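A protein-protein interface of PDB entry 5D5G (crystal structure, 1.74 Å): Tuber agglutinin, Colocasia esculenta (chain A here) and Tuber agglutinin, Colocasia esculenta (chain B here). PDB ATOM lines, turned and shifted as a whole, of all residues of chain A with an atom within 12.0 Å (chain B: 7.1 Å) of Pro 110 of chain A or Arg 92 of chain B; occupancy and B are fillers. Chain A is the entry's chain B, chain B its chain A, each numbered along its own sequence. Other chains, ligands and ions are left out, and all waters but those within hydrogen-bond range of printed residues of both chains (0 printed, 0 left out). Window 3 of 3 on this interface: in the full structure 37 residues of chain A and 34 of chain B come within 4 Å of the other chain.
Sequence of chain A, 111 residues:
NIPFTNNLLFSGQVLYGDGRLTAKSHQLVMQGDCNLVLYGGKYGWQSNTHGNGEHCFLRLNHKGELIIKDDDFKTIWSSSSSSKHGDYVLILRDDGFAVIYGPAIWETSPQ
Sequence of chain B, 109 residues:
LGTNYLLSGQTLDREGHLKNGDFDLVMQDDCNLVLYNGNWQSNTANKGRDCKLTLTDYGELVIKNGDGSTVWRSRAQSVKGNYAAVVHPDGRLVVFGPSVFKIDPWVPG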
ATOM      1  N   ASN A   1      -7.299  18.317  13.695  1.00  0.00           N
ATOM      2  CA  ASN A   1      -6.434  18.625  12.560  1.00  0.00           C
ATOM      3  C   ASN A   1      -5.288  17.660  12.331  1.00  0.00           C
ATOM      4  O   ASN A   1      -4.998  16.789  13.148  1.00  0.00           O
ATOM      5  CB  ASN A   1      -5.839  20.009  12.708  1.00  0.00           C
ATOM      6  CG  ASN A   1      -6.880  21.074  12.717  1.00  0.00           C
ATOM      7  OD1 ASN A   1      -7.909  20.929  13.361  1.00  0.00           O
ATOM      8  ND2 ASN A   1      -6.637  22.147  11.982  1.00  0.00           N
ATOM      9  N   ILE A   2      -4.602  17.882  11.222  1.00  0.00           N
ATOM     10  CA  ILE A   2      -3.660  16.927  10.690  1.00  0.00           C
ATOM     11  C   ILE A   2      -2.265  17.460  10.848  1.00  0.00           C
ATOM     12  O   ILE A   2      -1.972  18.574  10.425  1.00  0.00           O
ATOM     13  CB  ILE A   2      -3.928  16.676   9.192  1.00  0.00           C
ATOM     14  CG1 ILE A   2      -5.352  16.151   8.994  1.00  0.00           C
ATOM     15  CG2 ILE A   2      -2.919  15.698   8.607  1.00  0.00           C
ATOM     16  CD1 ILE A   2      -5.686  15.832   7.554  1.00  0.00           C
ATOM     17  N   PRO A   3      -1.400  16.656  11.463  1.00  0.00           N
ATOM     18  CA  PRO A   3      -0.001  16.976  11.738  1.00  0.00           C
ATOM     19  C   PRO A   3       0.687  17.398  10.474  1.00  0.00           C
ATOM     20  O   PRO A   3       0.656  16.670   9.482  1.00  0.00           O
ATOM     21  CB  PRO A   3       0.568  15.637  12.169  1.00  0.00           C
ATOM     22  CG  PRO A   3      -0.601  14.915  12.764  1.00  0.00           C
ATOM     23  CD  PRO A   3      -1.755  15.295  11.902  1.00  0.00           C
ATOM     24  N   THR A   5       3.349  17.933   7.676  1.00  0.00           N
ATOM     25  CA  THR A   5       4.604  17.306   7.270  1.00  0.00           C
ATOM     26  C   THR A   5       5.304  18.357   6.435  1.00  0.00           C
ATOM     27  O   THR A   5       4.651  19.163   5.787  1.00  0.00           O
ATOM     28  CB  THR A   5       4.423  15.987   6.473  1.00  0.00           C
ATOM     29  OG1 THR A   5       3.882  14.974   7.324  1.00  0.00           O
ATOM     30  CG2 THR A   5       5.748  15.486   5.950  1.00  0.00           C
ATOM     31  N   LEU A   8       4.491  18.054   2.349  1.00  0.00           N
ATOM     32  CA  LEU A   8       3.180  17.599   1.944  1.00  0.00           C
ATOM     33  C   LEU A   8       2.173  18.675   2.294  1.00  0.00           C
ATOM     34  O   LEU A   8       2.343  19.417   3.259  1.00  0.00           O
ATOM     35  CB  LEU A   8       2.828  16.312   2.691  1.00  0.00           C
ATOM     36  CG  LEU A   8       3.932  15.238   2.662  1.00  0.00           C
ATOM     37  CD1 LEU A   8       3.501  13.962   3.371  1.00  0.00           C
ATOM     38  CD2 LEU A   8       4.394  14.929   1.237  1.00  0.00           C
ATOM     39  N   PHE A  10      -1.782  17.958   2.506  1.00  0.00           N
ATOM     40  CA  PHE A  10      -2.921  17.111   2.255  1.00  0.00           C
ATOM     41  C   PHE A  10      -4.134  17.994   2.125  1.00  0.00           C
ATOM     42  O   PHE A  10      -4.122  19.153   2.527  1.00  0.00           O
ATOM     43  CB  PHE A  10      -3.122  16.116   3.398  1.00  0.00           C
ATOM     44  CG  PHE A  10      -2.019  15.092   3.512  1.00  0.00           C
ATOM     45  CD1 PHE A  10      -2.049  13.930   2.758  1.00  0.00           C
ATOM     46  CD2 PHE A  10      -0.955  15.297   4.381  1.00  0.00           C
ATOM     47  CE1 PHE A  10      -1.033  12.990   2.868  1.00  0.00           C
ATOM     48  CE2 PHE A  10       0.072  14.356   4.498  1.00  0.00           C
ATOM     49  CZ  PHE A  10       0.028  13.201   3.746  1.00  0.00           C
ATOM     50  N   SER A  11      -5.183  17.440   1.542  1.00  0.00           N
ATOM     51  CA  SER A  11      -6.428  18.163   1.404  1.00  0.00           C
ATOM     52  C   SER A  11      -6.916  18.573   2.781  1.00  0.00           C
ATOM     53  O   SER A  11      -6.756  17.831   3.751  1.00  0.00           O
ATOM     54  CB  SER A  11      -7.461  17.284   0.698  1.00  0.00           C
ATOM     55  OG  SER A  11      -6.951  16.827  -0.544  1.00  0.00           O
ATOM     56  N   HIS A  62     -11.024  18.470  -1.214  1.00  0.00           N
ATOM     57  CA  HIS A  62     -11.203  17.043  -1.492  1.00  0.00           C
ATOM     58  C   HIS A  62     -11.699  16.718  -2.901  1.00  0.00           C
ATOM     59  O   HIS A  62     -12.474  15.780  -3.085  1.00  0.00           O
ATOM     60  CB  HIS A  62     -12.146  16.419  -0.475  1.00  0.00           C
ATOM     61  CG  HIS A  62     -11.528  16.248   0.871  1.00  0.00           C
ATOM     62  ND1 HIS A  62     -11.410  17.285   1.769  1.00  0.00           N
ATOM     63  CD2 HIS A  62     -10.958  15.170   1.458  1.00  0.00           C
ATOM     64  CE1 HIS A  62     -10.808  16.851   2.861  1.00  0.00           C
ATOM     65  NE2 HIS A  62     -10.528  15.570   2.700  1.00  0.00           N
ATOM     66  N   GLY A  86     -12.371  12.947  -2.629  1.00  0.00           N
ATOM     67  CA  GLY A  86     -11.596  12.136  -1.723  1.00  0.00           C
ATOM     68  C   GLY A  86     -10.320  12.870  -1.434  1.00  0.00           C
ATOM     69  O   GLY A  86     -10.168  14.011  -1.855  1.00  0.00           O
ATOM     70  N   ASP A  87      -9.399  12.192  -0.752  1.00  0.00           N
ATOM     71  CA  ASP A  87      -8.184  12.795  -0.229  1.00  0.00           C
ATOM     72  C   ASP A  87      -7.116  12.945  -1.302  1.00  0.00           C
ATOM     73  O   ASP A  87      -6.810  12.006  -2.027  1.00  0.00           O
ATOM     74  CB  ASP A  87      -7.703  11.937   0.937  1.00  0.00           C
ATOM     75  CG  ASP A  87      -8.843  11.597   1.889  1.00  0.00           C
ATOM     76  OD1 ASP A  87     -10.002  11.904   1.527  1.00  0.00           O
ATOM     77  OD2 ASP A  87      -8.613  11.033   2.987  1.00  0.00           O
ATOM     78  N   TYR A  88      -6.589  14.156  -1.423  1.00  0.00           N
ATOM     79  CA  TYR A  88      -5.540  14.479  -2.380  1.00  0.00           C
ATOM     80  C   TYR A  88      -4.354  14.983  -1.573  1.00  0.00           C
ATOM     81  O   TYR A  88      -4.527  15.400  -0.426  1.00  0.00           O
ATOM     82  CB  TYR A  88      -6.005  15.606  -3.304  1.00  0.00           C
ATOM     83  CG  TYR A  88      -7.038  15.185  -4.322  1.00  0.00           C
ATOM     84  CD1 TYR A  88      -8.311  14.802  -3.932  1.00  0.00           C
ATOM     85  CD2 TYR A  88      -6.730  15.171  -5.670  1.00  0.00           C
ATOM     86  CE1 TYR A  88      -9.251  14.401  -4.868  1.00  0.00           C
ATOM     87  CE2 TYR A  88      -7.657  14.786  -6.610  1.00  0.00           C
ATOM     88  CZ  TYR A  88      -8.915  14.396  -6.207  1.00  0.00           C
ATOM     89  OH  TYR A  88      -9.838  13.998  -7.160  1.00  0.00           O
ATOM     90  N   VAL A  89      -3.165  14.975  -2.166  1.00  0.00           N
ATOM     91  CA  VAL A  89      -2.013  15.581  -1.509  1.00  0.00           C
ATOM     92  C   VAL A  89      -1.196  16.328  -2.538  1.00  0.00           C
ATOM     93  O   VAL A  89      -1.027  15.863  -3.667  1.00  0.00           O
ATOM     94  CB  VAL A  89      -1.135  14.540  -0.696  1.00  0.00           C
ATOM     95  CG1 VAL A  89      -0.492  13.486  -1.597  1.00  0.00           C
ATOM     96  CG2 VAL A  89      -0.054  15.232   0.123  1.00  0.00           C
ATOM     97  N   ILE A  91       2.592  17.613  -3.163  1.00  0.00           N
ATOM     98  CA  ILE A  91       3.931  17.298  -2.704  1.00  0.00           C
ATOM     99  C   ILE A  91       4.841  18.398  -3.205  1.00  0.00           C
ATOM    100  O   ILE A  91       4.597  18.925  -4.270  1.00  0.00           O
ATOM    101  CB  ILE A  91       4.386  15.942  -3.265  1.00  0.00           C
ATOM    102  CG1 ILE A  91       3.660  14.811  -2.541  1.00  0.00           C
ATOM    103  CG2 ILE A  91       5.884  15.767  -3.131  1.00  0.00           C
ATOM    104  CD1 ILE A  91       3.711  13.507  -3.270  1.00  0.00           C
ATOM    105  N   PRO A 103      -7.310  10.801  -6.275  1.00  0.00           N
ATOM    106  CA  PRO A 103      -7.433  10.614  -4.834  1.00  0.00           C
ATOM    107  C   PRO A 103      -6.811   9.316  -4.313  1.00  0.00           C
ATOM    108  O   PRO A 103      -6.098   8.592  -5.018  1.00  0.00           O
ATOM    109  CB  PRO A 103      -8.944  10.542  -4.643  1.00  0.00           C
ATOM    110  CG  PRO A 103      -9.411   9.865  -5.860  1.00  0.00           C
ATOM    111  CD  PRO A 103      -8.522  10.369  -6.979  1.00  0.00           C
ATOM    112  N   ALA A 104      -7.112   9.033  -3.050  1.00  0.00           N
ATOM    113  CA  ALA A 104      -6.631   7.830  -2.400  1.00  0.00           C
ATOM    114  C   ALA A 104      -7.269   6.620  -3.042  1.00  0.00           C
ATOM    115  O   ALA A 104      -8.442   6.332  -2.818  1.00  0.00           O
ATOM    116  CB  ALA A 104      -6.962   7.869  -0.930  1.00  0.00           C
ATOM    117  N   ILE A 105      -6.492   5.898  -3.833  1.00  0.00           N
ATOM    118  CA  ILE A 105      -6.992   4.676  -4.441  1.00  0.00           C
ATOM    119  C   ILE A 105      -6.532   3.427  -3.689  1.00  0.00           C
ATOM    120  O   ILE A 105      -6.930   2.306  -4.023  1.00  0.00           O
ATOM    121  CB  ILE A 105      -6.541   4.568  -5.899  1.00  0.00           C
ATOM    122  CG1 ILE A 105      -5.025   4.356  -5.957  1.00  0.00           C
ATOM    123  CG2 ILE A 105      -6.976   5.806  -6.678  1.00  0.00           C
ATOM    124  CD1 ILE A 105      -4.459   4.274  -7.356  1.00  0.00           C
ATOM    125  N   TRP A 106      -5.688   3.618  -2.682  1.00  0.00           N
ATOM    126  CA  TRP A 106      -5.226   2.507  -1.858  1.00  0.00           C
ATOM    127  C   TRP A 106      -4.520   3.023  -0.622  1.00  0.00           C
ATOM    128  O   TRP A 106      -3.584   3.825  -0.724  1.00  0.00           O
ATOM    129  CB  TRP A 106      -4.296   1.585  -2.645  1.00  0.00           C
ATOM    130  CG  TRP A 106      -4.080   0.254  -1.987  1.00  0.00           C
ATOM    131  CD1 TRP A 106      -4.840  -0.873  -2.136  1.00  0.00           C
ATOM    132  CD2 TRP A 106      -3.033  -0.088  -1.077  1.00  0.00           C
ATOM    133  NE1 TRP A 106      -4.326  -1.894  -1.372  1.00  0.00           N
ATOM    134  CE2 TRP A 106      -3.219  -1.433  -0.708  1.00  0.00           C
ATOM    135  CE3 TRP A 106      -1.956   0.618  -0.531  1.00  0.00           C
ATOM    136  CZ2 TRP A 106      -2.371  -2.084   0.177  1.00  0.00           C
ATOM    137  CZ3 TRP A 106      -1.118  -0.028   0.348  1.00  0.00           C
ATOM    138  CH2 TRP A 106      -1.328  -1.365   0.694  1.00  0.00           C
ATOM    139  N   GLU A 107      -4.992   2.561   0.535  1.00  0.00           N
ATOM    140  CA  GLU A 107      -4.384   2.874   1.822  1.00  0.00           C
ATOM    141  C   GLU A 107      -4.130   1.578   2.610  1.00  0.00           C
ATOM    142  O   GLU A 107      -4.738   0.549   2.312  1.00  0.00           O
ATOM    143  CB  GLU A 107      -5.275   3.826   2.617  1.00  0.00           C
ATOM    144  CG  GLU A 107      -6.563   3.218   3.128  1.00  0.00           C
ATOM    145  CD  GLU A 107      -7.422   4.255   3.811  1.00  0.00           C
ATOM    146  OE1 GLU A 107      -8.253   3.895   4.671  1.00  0.00           O
ATOM    147  OE2 GLU A 107      -7.258   5.445   3.479  1.00  0.00           O
ATOM    148  N   THR A 108      -3.241   1.634   3.607  1.00  0.00           N
ATOM    149  CA  THR A 108      -2.821   0.446   4.348  1.00  0.00           C
ATOM    150  C   THR A 108      -3.794  -0.036   5.424  1.00  0.00           C
ATOM    151  O   THR A 108      -3.686  -1.170   5.881  1.00  0.00           O
ATOM    152  CB  THR A 108      -1.476   0.680   5.011  1.00  0.00           C
ATOM    153  OG1 THR A 108      -1.499   1.937   5.699  1.00  0.00           O
ATOM    154  CG2 THR A 108      -0.398   0.718   3.964  1.00  0.00           C
ATOM    155  N   SER A 109      -4.710   0.835   5.838  1.00  0.00           N
ATOM    156  CA  SER A 109      -5.842   0.480   6.711  1.00  0.00           C
ATOM    157  C   SER A 109      -6.739   1.699   7.001  1.00  0.00           C
ATOM    158  O   SER A 109      -6.271   2.840   6.972  1.00  0.00           O
ATOM    159  CB  SER A 109      -5.377  -0.171   8.017  1.00  0.00           C
ATOM    160  OG  SER A 109      -4.968  -1.506   7.778  1.00  0.00           O
ATOM    161  N   PRO A 110      -8.042   1.465   7.263  1.00  0.00           N
ATOM    162  CA  PRO A 110      -8.932   2.586   7.599  1.00  0.00           C
ATOM    163  C   PRO A 110      -9.128   2.744   9.106  1.00  0.00           C
ATOM    164  O   PRO A 110     -10.046   2.140   9.670  1.00  0.00           O
ATOM    165  CB  PRO A 110     -10.264   2.191   6.938  1.00  0.00           C
ATOM    166  CG  PRO A 110     -10.098   0.716   6.493  1.00  0.00           C
ATOM    167  CD  PRO A 110      -8.803   0.219   7.087  1.00  0.00           C
ATOM    168  N   PHE B  23       6.389   6.549  12.167  1.00  0.00           N
ATOM    169  CA  PHE B  23       6.040   5.425  11.300  1.00  0.00           C
ATOM    170  C   PHE B  23       7.126   5.144  10.280  1.00  0.00           C
ATOM    171  O   PHE B  23       7.498   6.026   9.489  1.00  0.00           O
ATOM    172  CB  PHE B  23       4.694   5.656  10.622  1.00  0.00           C
ATOM    173  CG  PHE B  23       3.581   5.932  11.587  1.00  0.00           C
ATOM    174  CD1 PHE B  23       2.961   4.891  12.271  1.00  0.00           C
ATOM    175  CD2 PHE B  23       3.161   7.240  11.829  1.00  0.00           C
ATOM    176  CE1 PHE B  23       1.933   5.143  13.170  1.00  0.00           C
ATOM    177  CE2 PHE B  23       2.136   7.503  12.716  1.00  0.00           C
ATOM    178  CZ  PHE B  23       1.515   6.454  13.395  1.00  0.00           C
ATOM    179  N   LEU B  35       5.625  -1.687   7.548  1.00  0.00           N
ATOM    180  CA  LEU B  35       5.445  -0.305   7.951  1.00  0.00           C
ATOM    181  C   LEU B  35       5.415  -0.303   9.475  1.00  0.00           C
ATOM    182  O   LEU B  35       4.411  -0.674  10.071  1.00  0.00           O
ATOM    183  CB  LEU B  35       4.128   0.212   7.362  1.00  0.00           C
ATOM    184  CG  LEU B  35       3.618   1.620   7.651  1.00  0.00           C
ATOM    185  CD1 LEU B  35       4.342   2.654   6.810  1.00  0.00           C
ATOM    186  CD2 LEU B  35       2.120   1.674   7.386  1.00  0.00           C
ATOM    187  N   GLY B  38       2.779   1.082  11.920  1.00  0.00           N
ATOM    188  CA  GLY B  38       1.614   0.810  11.097  1.00  0.00           C
ATOM    189  C   GLY B  38       1.356  -0.672  11.302  1.00  0.00           C
ATOM    190  O   GLY B  38       2.275  -1.490  11.237  1.00  0.00           O
ATOM    191  N   VAL B  86       2.665   7.558  -0.366  1.00  0.00           N
ATOM    192  CA  VAL B  86       3.240   8.424   0.645  1.00  0.00           C
ATOM    193  C   VAL B  86       2.868   7.963   2.045  1.00  0.00           C
ATOM    194  O   VAL B  86       1.752   7.484   2.272  1.00  0.00           O
ATOM    195  CB  VAL B  86       2.799   9.848   0.427  1.00  0.00           C
ATOM    196  CG1 VAL B  86       3.470  10.418  -0.807  1.00  0.00           C
ATOM    197  CG2 VAL B  86       1.314   9.885   0.261  1.00  0.00           C
ATOM    198  N   VAL B  87       3.818   8.074   2.979  1.00  0.00           N
ATOM    199  CA  VAL B  87       3.562   7.707   4.374  1.00  0.00           C
ATOM    200  C   VAL B  87       2.826   8.844   5.091  1.00  0.00           C
ATOM    201  O   VAL B  87       3.396   9.907   5.395  1.00  0.00           O
ATOM    202  CB  VAL B  87       4.859   7.360   5.151  1.00  0.00           C
ATOM    203  CG1 VAL B  87       4.521   6.537   6.389  1.00  0.00           C
ATOM    204  CG2 VAL B  87       5.823   6.596   4.265  1.00  0.00           C
ATOM    205  N   HIS B  88       1.548   8.619   5.357  1.00  0.00           N
ATOM    206  CA  HIS B  88       0.736   9.636   5.980  1.00  0.00           C
ATOM    207  C   HIS B  88       1.090   9.785   7.440  1.00  0.00           C
ATOM    208  O   HIS B  88       1.237   8.791   8.143  1.00  0.00           O
ATOM    209  CB  HIS B  88      -0.721   9.254   5.886  1.00  0.00           C
ATOM    210  CG  HIS B  88      -1.647  10.326   6.349  1.00  0.00           C
ATOM    211  ND1 HIS B  88      -1.862  11.485   5.633  1.00  0.00           N
ATOM    212  CD2 HIS B  88      -2.420  10.415   7.454  1.00  0.00           C
ATOM    213  CE1 HIS B  88      -2.733  12.237   6.277  1.00  0.00           C
ATOM    214  NE2 HIS B  88      -3.087  11.612   7.388  1.00  0.00           N
ATOM    215  N   PRO B  89       1.193  11.032   7.908  1.00  0.00           N
ATOM    216  CA  PRO B  89       1.551  11.310   9.299  1.00  0.00           C
ATOM    217  C   PRO B  89       0.596  10.649  10.289  1.00  0.00           C
ATOM    218  O   PRO B  89       0.978  10.479  11.442  1.00  0.00           O
ATOM    219  CB  PRO B  89       1.468  12.842   9.389  1.00  0.00           C
ATOM    220  CG  PRO B  89       0.675  13.275   8.191  1.00  0.00           C
ATOM    221  CD  PRO B  89       0.991  12.270   7.136  1.00  0.00           C
ATOM    222  N   ASP B  90      -0.609  10.264   9.869  1.00  0.00           N
ATOM    223  CA  ASP B  90      -1.467   9.517  10.793  1.00  0.00           C
ATOM    224  C   ASP B  90      -1.161   8.030  10.710  1.00  0.00           C
ATOM    225  O   ASP B  90      -1.828   7.205  11.330  1.00  0.00           O
ATOM    226  CB  ASP B  90      -2.954   9.791  10.582  1.00  0.00           C
ATOM    227  CG  ASP B  90      -3.339  11.225  10.917  1.00  0.00           C
ATOM    228  OD1 ASP B  90      -3.291  11.610  12.114  1.00  0.00           O
ATOM    229  OD2 ASP B  90      -3.694  11.973   9.982  1.00  0.00           O
ATOM    230  N   GLY B  91      -0.143   7.691   9.934  1.00  0.00           N
ATOM    231  CA  GLY B  91       0.386   6.336   9.973  1.00  0.00           C
ATOM    232  C   GLY B  91      -0.138   5.334   8.963  1.00  0.00           C
ATOM    233  O   GLY B  91      -0.192   4.150   9.263  1.00  0.00           O
ATOM    234  N   ARG B  92      -0.513   5.787   7.771  1.00  0.00           N
ATOM    235  CA  ARG B  92      -0.864   4.854   6.707  1.00  0.00           C
ATOM    236  C   ARG B  92       0.056   5.066   5.525  1.00  0.00           C
ATOM    237  O   ARG B  92       0.561   6.163   5.309  1.00  0.00           O
ATOM    238  CB  ARG B  92      -2.282   5.091   6.235  1.00  0.00           C
ATOM    239  CG  ARG B  92      -3.376   4.851   7.247  1.00  0.00           C
ATOM    240  CD  ARG B  92      -4.675   5.398   6.660  1.00  0.00           C
ATOM    241  NE  ARG B  92      -5.845   5.168   7.506  1.00  0.00           N
ATOM    242  CZ  ARG B  92      -6.503   6.130   8.150  1.00  0.00           C
ATOM    243  NH1 ARG B  92      -6.104   7.394   8.051  1.00  0.00           N
ATOM    244  NH2 ARG B  92      -7.566   5.834   8.892  1.00  0.00           N
ATOM    245  N   LEU B  93       0.286   4.014   4.751  1.00  0.00           N
ATOM    246  CA  LEU B  93       0.870   4.220   3.437  1.00  0.00           C
ATOM    247  C   LEU B  93      -0.296   4.295   2.457  1.00  0.00           C
ATOM    248  O   LEU B  93      -1.100   3.360   2.386  1.00  0.00           O
ATOM    249  CB  LEU B  93       1.813   3.093   3.063  1.00  0.00           C
ATOM    250  CG  LEU B  93       2.485   3.278   1.711  1.00  0.00           C
ATOM    251  CD1 LEU B  93       3.433   4.449   1.737  1.00  0.00           C
ATOM    252  CD2 LEU B  93       3.224   2.014   1.356  1.00  0.00           C
ATOM    253  N   VAL B  94      -0.407   5.412   1.734  1.00  0.00           N
ATOM    254  CA  VAL B  94      -1.552   5.647   0.831  1.00  0.00           C
ATOM    255  C   VAL B  94      -1.112   6.004  -0.588  1.00  0.00           C
ATOM    256  O   VAL B  94      -0.353   6.950  -0.782  1.00  0.00           O
ATOM    257  CB  VAL B  94      -2.447   6.789   1.343  1.00  0.00           C
ATOM    258  CG1 VAL B  94      -3.646   6.969   0.424  1.00  0.00           C
ATOM    259  CG2 VAL B  94      -2.909   6.514   2.764  1.00  0.00           C
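The backbone NH (N) of Val 94 of chain B sits at hydrogen-bond distance from the backbone carbonyl oxygen (O) of Val 86 of chain B (3.0 Å).
NE2 of His 88 of chain B is in hydrogen-bond range of OD2 of Asp 90 of chain B, 2.7 Å away.
The backbone NH (N) of Ala 104 of chain A sits at hydrogen-bond distance from the backbone carbonyl oxygen (O) of Asp 87 of chain A (3.2 Å).
Tyr 88 of chain A touches none of the printed residues of chain B.
Pro 103 of chain A touches none of the printed residues of chain B.
Of the printed residues of chain B, Trp 106 of chain A touches Leu 93 (3.95 Å) and Val 94 (3.1 Å).
Printed residues of chain B within 4 Å of Glu 107 of chain A: Arg 92, Leu 93 and Val 94.
Of the printed residues of chain B, Pro 110 of chain A touches Arg 92.
Val 87 of chain B touches none of the printed residues of chain A.
Of chain A, only Phe 10 comes within 4 Å of His 88 of chain B.
Of chain A, only Pro 3, Thr 5 and Phe 10 come within 4 Å of Pro 89 of chain B.
No residue of chain A comes within 4 Å of Gly 91 of chain B.
Of chain A, only Glu 107, Thr 108, Ser 109 and Pro 110 come within 4 Å of Arg 92 of chain B.
Pro 3 of chain A touches Pro 89 of chain B.
OD1 of Asp 90 of chain B touches CD of Pro 3 of chain A (3.998 Å).
Thr 5 of chain A touches Pro 89 of chain B (OG1 to CG, 3.7 Å).
His 88 of chain B touches Phe 10 of chain A (ND1 to CZ, 3.2 Å).
Ile 91 of chain A touches Val 86 of chain B.
O of Leu 93 of chain B touches CZ3 of Trp 106 of chain A, at 3.95 Å.
CA of Glu 107 of chain A touches O of Leu 93 of chain B (3.4 Å).
CB of Glu 107 of chain A touches CG2 of Val 94 of chain B, at 3.6 Å.
CA of Arg 92 of chain B touches OG1 of Thr 108 of chain A (3.2 Å).
C of Pro 110 of chain A touches NH2 of Arg 92 of chain B, at 3.5 Å.
The side-chain carboxylate (OE1) of Glu 107 of chain A lies within salt-bridge range of the guanidinium group (NE) of Arg 92 of chain B (3.9 Å).
O of Ser 109 of chain A lies within hydrogen-bond range of NE of Arg 92 of chain B (2.4 Å).
N of Leu 93 of chain B lies within hydrogen-bond range of OG1 of Thr 108 of chain A, at 2.9 Å.
Along chain A the printed residues that touch a printed residue of chain B span positions 3 to 110.
Printed residues of chain B that touch a printed residue of chain A: Val 86, His 88, Pro 89, Asp 90, Arg 92, Leu 93 and Val 94.
Along chain B the printed residues that touch a printed residue of chain A span positions 86 to 94.
Among the printed residues, 16 pairs touch across the chains.
Among the printed residues, Asp or Glu carboxylates within 4 Å of a Lys or Arg side-chain nitrogen of the other chain: Glu 107 of chain A with Arg 92 of chain B (3.9 Å).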
